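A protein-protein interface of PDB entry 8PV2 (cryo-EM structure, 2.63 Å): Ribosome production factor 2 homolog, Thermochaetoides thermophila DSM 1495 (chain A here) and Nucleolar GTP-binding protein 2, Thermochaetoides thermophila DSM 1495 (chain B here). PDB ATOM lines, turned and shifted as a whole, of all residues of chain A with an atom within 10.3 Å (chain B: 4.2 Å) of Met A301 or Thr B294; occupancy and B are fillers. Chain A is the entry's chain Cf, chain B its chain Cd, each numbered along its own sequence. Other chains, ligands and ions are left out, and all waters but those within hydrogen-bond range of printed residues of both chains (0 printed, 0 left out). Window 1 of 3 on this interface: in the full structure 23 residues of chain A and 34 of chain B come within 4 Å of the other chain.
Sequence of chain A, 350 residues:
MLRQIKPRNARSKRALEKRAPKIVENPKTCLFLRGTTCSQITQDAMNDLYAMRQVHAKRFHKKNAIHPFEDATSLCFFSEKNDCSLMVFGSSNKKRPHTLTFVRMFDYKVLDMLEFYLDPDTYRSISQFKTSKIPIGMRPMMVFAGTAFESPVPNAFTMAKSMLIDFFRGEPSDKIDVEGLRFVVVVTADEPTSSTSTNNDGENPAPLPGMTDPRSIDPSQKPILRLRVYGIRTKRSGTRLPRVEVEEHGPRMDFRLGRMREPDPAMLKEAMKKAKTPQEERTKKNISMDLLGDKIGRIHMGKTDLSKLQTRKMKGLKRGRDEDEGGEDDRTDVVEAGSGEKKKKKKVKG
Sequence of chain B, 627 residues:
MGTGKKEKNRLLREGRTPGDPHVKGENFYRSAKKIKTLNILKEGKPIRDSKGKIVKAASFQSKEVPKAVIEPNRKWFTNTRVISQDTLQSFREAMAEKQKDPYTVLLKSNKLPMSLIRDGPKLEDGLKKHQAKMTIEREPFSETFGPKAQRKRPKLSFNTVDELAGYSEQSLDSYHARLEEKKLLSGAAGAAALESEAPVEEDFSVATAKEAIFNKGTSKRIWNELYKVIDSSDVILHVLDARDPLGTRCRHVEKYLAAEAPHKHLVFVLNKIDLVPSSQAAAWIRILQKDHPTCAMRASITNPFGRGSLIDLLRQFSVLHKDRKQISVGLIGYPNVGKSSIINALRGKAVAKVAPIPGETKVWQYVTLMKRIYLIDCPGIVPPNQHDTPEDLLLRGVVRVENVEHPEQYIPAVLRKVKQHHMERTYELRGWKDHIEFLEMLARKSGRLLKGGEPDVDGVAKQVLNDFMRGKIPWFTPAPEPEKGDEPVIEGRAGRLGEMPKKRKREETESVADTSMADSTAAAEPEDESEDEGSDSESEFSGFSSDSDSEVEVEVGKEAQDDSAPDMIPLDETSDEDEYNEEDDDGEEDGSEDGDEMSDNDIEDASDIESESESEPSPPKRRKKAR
The backbone NH (N) of Phe B268 is in hydrogen-bond range of the backbone carbonyl oxygen (O) of Pro B293.
The backbone carbonyl oxygen (O) of His B292 is in hydrogen-bond range of the side-chain hydroxyl (OG1) of Thr B294, 2.9 Å away.
Printed residues of chain B within 4 Å of Ile A299: Pro B293 (3.7 Å).
Lys A303 touches none of the printed residues of chain B.
No residue of chain A comes within 4 Å of Leu B288.
Gln B289 touches none of the printed residues of chain A.
His B292 touches none of the printed residues of chain A.
Thr B294 touches one residue of chain A.
Printed residues of chain A within 4 Å of Leu B313: Met A301.
The nearest printed residue of chain B that does not touch Ile A299 is Leu B313 (4.02 Å).
Among the printed residues, merely in contact across the chains: Ile A299 with Pro B293, Met A301 with Pro B293, Met A301 with Thr B294 and Met A301 with Leu B313.
Of the 10 printed residues of chain A, 2 touch a printed residue of chain B.
Hydrophobic or aromatic side chains of chain A that line the printed part of chain B: Ile A299 and Met A301.
Printed residues of chain B that touch a printed residue of chain A: Pro B293, Thr B294 and Leu B313.
Among the printed residues, no Asp or Glu carboxylate lies within 4 Å of a Lys or Arg side-chain nitrogen of the other chain.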
ATOM      1  N   ASN A 286      38.419   2.199   9.927  1.00  0.00           N
ATOM      2  CA  ASN A 286      37.791   1.623  11.116  1.00  0.00           C
ATOM      3  C   ASN A 286      38.600   0.499  11.751  1.00  0.00           C
ATOM      4  O   ASN A 286      38.067  -0.241  12.580  1.00  0.00           O
ATOM      5  CB  ASN A 286      36.372   1.121  10.823  1.00  0.00           C
ATOM      6  CG  ASN A 286      35.442   2.226  10.415  1.00  0.00           C
ATOM      7  OD1 ASN A 286      35.493   3.323  10.963  1.00  0.00           O
ATOM      8  ND2 ASN A 286      34.592   1.951   9.438  1.00  0.00           N
ATOM      9  N   ARG A 298      35.793  -0.639  14.484  1.00  0.00           N
ATOM     10  CA  ARG A 298      34.809   0.361  14.877  1.00  0.00           C
ATOM     11  C   ARG A 298      33.530   0.163  14.079  1.00  0.00           C
ATOM     12  O   ARG A 298      33.567   0.084  12.848  1.00  0.00           O
ATOM     13  CB  ARG A 298      35.338   1.774  14.650  1.00  0.00           C
ATOM     14  CG  ARG A 298      35.881   2.429  15.889  1.00  0.00           C
ATOM     15  CD  ARG A 298      34.776   2.978  16.763  1.00  0.00           C
ATOM     16  NE  ARG A 298      35.329   3.684  17.911  1.00  0.00           N
ATOM     17  CZ  ARG A 298      34.609   4.167  18.915  1.00  0.00           C
ATOM     18  NH1 ARG A 298      33.295   4.033  18.949  1.00  0.00           N
ATOM     19  NH2 ARG A 298      35.226   4.793  19.912  1.00  0.00           N
ATOM     20  N   ILE A 299      32.405   0.087  14.781  1.00  0.00           N
ATOM     21  CA  ILE A 299      31.097   0.001  14.150  1.00  0.00           C
ATOM     22  C   ILE A 299      30.338   1.276  14.469  1.00  0.00           C
ATOM     23  O   ILE A 299      30.632   1.964  15.451  1.00  0.00           O
ATOM     24  CB  ILE A 299      30.304  -1.239  14.606  1.00  0.00           C
ATOM     25  CG1 ILE A 299      30.103  -1.214  16.117  1.00  0.00           C
ATOM     26  CG2 ILE A 299      31.022  -2.505  14.186  1.00  0.00           C
ATOM     27  CD1 ILE A 299      29.204  -2.299  16.612  1.00  0.00           C
ATOM     28  N   HIS A 300      29.361   1.597  13.628  1.00  0.00           N
ATOM     29  CA  HIS A 300      28.637   2.862  13.713  1.00  0.00           C
ATOM     30  C   HIS A 300      27.144   2.591  13.606  1.00  0.00           C
ATOM     31  O   HIS A 300      26.642   2.269  12.524  1.00  0.00           O
ATOM     32  CB  HIS A 300      29.122   3.820  12.631  1.00  0.00           C
ATOM     33  CG  HIS A 300      30.607   3.989  12.615  1.00  0.00           C
ATOM     34  ND1 HIS A 300      31.270   4.816  13.494  1.00  0.00           N
ATOM     35  CD2 HIS A 300      31.562   3.413  11.849  1.00  0.00           C
ATOM     36  CE1 HIS A 300      32.567   4.751  13.263  1.00  0.00           C
ATOM     37  NE2 HIS A 300      32.772   3.909  12.268  1.00  0.00           N
ATOM     38  N   MET A 301      26.437   2.730  14.728  1.00  0.00           N
ATOM     39  CA  MET A 301      25.026   2.362  14.780  1.00  0.00           C
ATOM     40  C   MET A 301      24.149   3.383  14.068  1.00  0.00           C
ATOM     41  O   MET A 301      23.191   3.019  13.379  1.00  0.00           O
ATOM     42  CB  MET A 301      24.582   2.205  16.232  1.00  0.00           C
ATOM     43  CG  MET A 301      25.323   1.129  16.989  1.00  0.00           C
ATOM     44  SD  MET A 301      25.174  -0.465  16.177  1.00  0.00           S
ATOM     45  CE  MET A 301      23.442  -0.805  16.466  1.00  0.00           C
ATOM     46  N   GLY A 302      24.451   4.661  14.231  1.00  0.00           N
ATOM     47  CA  GLY A 302      23.573   5.699  13.742  1.00  0.00           C
ATOM     48  C   GLY A 302      22.529   6.092  14.775  1.00  0.00           C
ATOM     49  O   GLY A 302      22.355   5.447  15.810  1.00  0.00           O
ATOM     50  N   LYS A 303      21.828   7.183  14.484  1.00  0.00           N
ATOM     51  CA  LYS A 303      20.820   7.689  15.405  1.00  0.00           C
ATOM     52  C   LYS A 303      19.581   6.802  15.389  1.00  0.00           C
ATOM     53  O   LYS A 303      19.146   6.333  14.333  1.00  0.00           O
ATOM     54  CB  LYS A 303      20.445   9.125  15.043  1.00  0.00           C
ATOM     55  N   THR A 304      19.015   6.571  16.571  1.00  0.00           N
ATOM     56  CA  THR A 304      17.787   5.798  16.692  1.00  0.00           C
ATOM     57  C   THR A 304      16.593   6.723  16.502  1.00  0.00           C
ATOM     58  O   THR A 304      16.298   7.551  17.370  1.00  0.00           O
ATOM     59  CB  THR A 304      17.717   5.106  18.051  1.00  0.00           C
ATOM     60  N   ASP A 305      15.904   6.582  15.371  1.00  0.00           N
ATOM     61  CA  ASP A 305      14.765   7.431  15.029  1.00  0.00           C
ATOM     62  C   ASP A 305      13.529   6.546  14.928  1.00  0.00           C
ATOM     63  O   ASP A 305      13.286   5.924  13.890  1.00  0.00           O
ATOM     64  CB  ASP A 305      15.010   8.192  13.731  1.00  0.00           C
ATOM     65  N   LEU A 306      12.753   6.496  16.003  1.00  0.00           N
ATOM     66  CA  LEU A 306      11.522   5.725  16.052  1.00  0.00           C
ATOM     67  C   LEU A 306      10.289   6.569  15.770  1.00  0.00           C
ATOM     68  O   LEU A 306       9.176   6.134  16.072  1.00  0.00           O
ATOM     69  CB  LEU A 306      11.379   5.046  17.416  1.00  0.00           C
ATOM     70  CG  LEU A 306      11.826   3.591  17.582  1.00  0.00           C
ATOM     71  CD1 LEU A 306      13.191   3.337  16.989  1.00  0.00           C
ATOM     72  CD2 LEU A 306      11.827   3.240  19.046  1.00  0.00           C
ATOM     73  N   PHE B 268      22.548  -6.770  20.515  1.00  0.00           N
ATOM     74  CA  PHE B 268      21.158  -6.867  20.938  1.00  0.00           C
ATOM     75  C   PHE B 268      20.232  -6.429  19.814  1.00  0.00           C
ATOM     76  O   PHE B 268      20.459  -5.405  19.168  1.00  0.00           O
ATOM     77  CB  PHE B 268      20.891  -6.004  22.170  1.00  0.00           C
ATOM     78  CG  PHE B 268      21.420  -6.579  23.443  1.00  0.00           C
ATOM     79  CD1 PHE B 268      21.295  -7.926  23.714  1.00  0.00           C
ATOM     80  CD2 PHE B 268      22.026  -5.764  24.382  1.00  0.00           C
ATOM     81  CE1 PHE B 268      21.776  -8.453  24.891  1.00  0.00           C
ATOM     82  CE2 PHE B 268      22.507  -6.283  25.561  1.00  0.00           C
ATOM     83  CZ  PHE B 268      22.382  -7.630  25.815  1.00  0.00           C
ATOM     84  N   LEU B 288      20.155  -0.662  27.135  1.00  0.00           N
ATOM     85  CA  LEU B 288      20.895  -1.806  26.602  1.00  0.00           C
ATOM     86  C   LEU B 288      22.188  -1.395  25.904  1.00  0.00           C
ATOM     87  O   LEU B 288      23.135  -2.194  25.829  1.00  0.00           O
ATOM     88  CB  LEU B 288      20.015  -2.595  25.636  1.00  0.00           C
ATOM     89  CG  LEU B 288      18.831  -3.332  26.255  1.00  0.00           C
ATOM     90  CD1 LEU B 288      17.846  -3.737  25.179  1.00  0.00           C
ATOM     91  CD2 LEU B 288      19.303  -4.536  27.039  1.00  0.00           C
ATOM     92  N   GLN B 289      22.252  -0.171  25.383  1.00  0.00           N
ATOM     93  CA  GLN B 289      23.435   0.251  24.648  1.00  0.00           C
ATOM     94  C   GLN B 289      24.618   0.560  25.552  1.00  0.00           C
ATOM     95  O   GLN B 289      25.728   0.743  25.044  1.00  0.00           O
ATOM     96  CB  GLN B 289      23.104   1.460  23.783  1.00  0.00           C
ATOM     97  CG  GLN B 289      22.396   1.081  22.506  1.00  0.00           C
ATOM     98  CD  GLN B 289      22.394   2.192  21.489  1.00  0.00           C
ATOM     99  OE1 GLN B 289      22.634   1.962  20.304  1.00  0.00           O
ATOM    100  NE2 GLN B 289      22.121   3.409  21.944  1.00  0.00           N
ATOM    101  N   HIS B 292      25.740  -3.446  25.056  1.00  0.00           N
ATOM    102  CA  HIS B 292      26.012  -3.962  23.725  1.00  0.00           C
ATOM    103  C   HIS B 292      25.265  -3.136  22.693  1.00  0.00           C
ATOM    104  O   HIS B 292      24.242  -2.523  23.017  1.00  0.00           O
ATOM    105  CB  HIS B 292      25.610  -5.442  23.623  1.00  0.00           C
ATOM    106  CG  HIS B 292      26.509  -6.355  24.393  1.00  0.00           C
ATOM    107  ND1 HIS B 292      26.242  -6.741  25.688  1.00  0.00           N
ATOM    108  CD2 HIS B 292      27.687  -6.932  24.062  1.00  0.00           C
ATOM    109  CE1 HIS B 292      27.207  -7.535  26.114  1.00  0.00           C
ATOM    110  NE2 HIS B 292      28.094  -7.669  25.146  1.00  0.00           N
ATOM    111  N   PRO B 293      25.767  -3.070  21.458  1.00  0.00           N
ATOM    112  CA  PRO B 293      25.064  -2.315  20.414  1.00  0.00           C
ATOM    113  C   PRO B 293      23.695  -2.909  20.134  1.00  0.00           C
ATOM    114  O   PRO B 293      23.553  -4.113  19.920  1.00  0.00           O
ATOM    115  CB  PRO B 293      25.993  -2.440  19.203  1.00  0.00           C
ATOM    116  CG  PRO B 293      27.305  -2.759  19.758  1.00  0.00           C
ATOM    117  CD  PRO B 293      27.071  -3.563  20.982  1.00  0.00           C
ATOM    118  N   THR B 294      22.681  -2.052  20.145  1.00  0.00           N
ATOM    119  CA  THR B 294      21.294  -2.486  20.125  1.00  0.00           C
ATOM    120  C   THR B 294      20.575  -1.881  18.933  1.00  0.00           C
ATOM    121  O   THR B 294      20.687  -0.682  18.668  1.00  0.00           O
ATOM    122  CB  THR B 294      20.586  -2.103  21.427  1.00  0.00           C
ATOM    123  OG1 THR B 294      21.339  -2.612  22.531  1.00  0.00           O
ATOM    124  CG2 THR B 294      19.180  -2.675  21.480  1.00  0.00           C
ATOM    125  N   CYS B 295      19.850  -2.727  18.211  1.00  0.00           N
ATOM    126  CA  CYS B 295      19.033  -2.321  17.080  1.00  0.00           C
ATOM    127  C   CYS B 295      17.573  -2.632  17.371  1.00  0.00           C
ATOM    128  O   CYS B 295      17.239  -3.754  17.753  1.00  0.00           O
ATOM    129  CB  CYS B 295      19.474  -3.041  15.803  1.00  0.00           C
ATOM    130  SG  CYS B 295      18.935  -2.254  14.274  1.00  0.00           S
ATOM    131  N   LEU B 313      24.539  -2.562   9.657  1.00  0.00           N
ATOM    132  CA  LEU B 313      25.452  -3.042  10.692  1.00  0.00           C
ATOM    133  C   LEU B 313      26.113  -4.361  10.286  1.00  0.00           C
ATOM    134  O   LEU B 313      27.321  -4.556  10.492  1.00  0.00           O
ATOM    135  CB  LEU B 313      24.709  -3.192  12.016  1.00  0.00           C
ATOM    136  CG  LEU B 313      25.576  -3.610  13.200  1.00  0.00           C
ATOM    137  CD1 LEU B 313      26.746  -2.655  13.370  1.00  0.00           C
ATOM    138  CD2 LEU B 313      24.756  -3.689  14.466  1.00  0.00           C
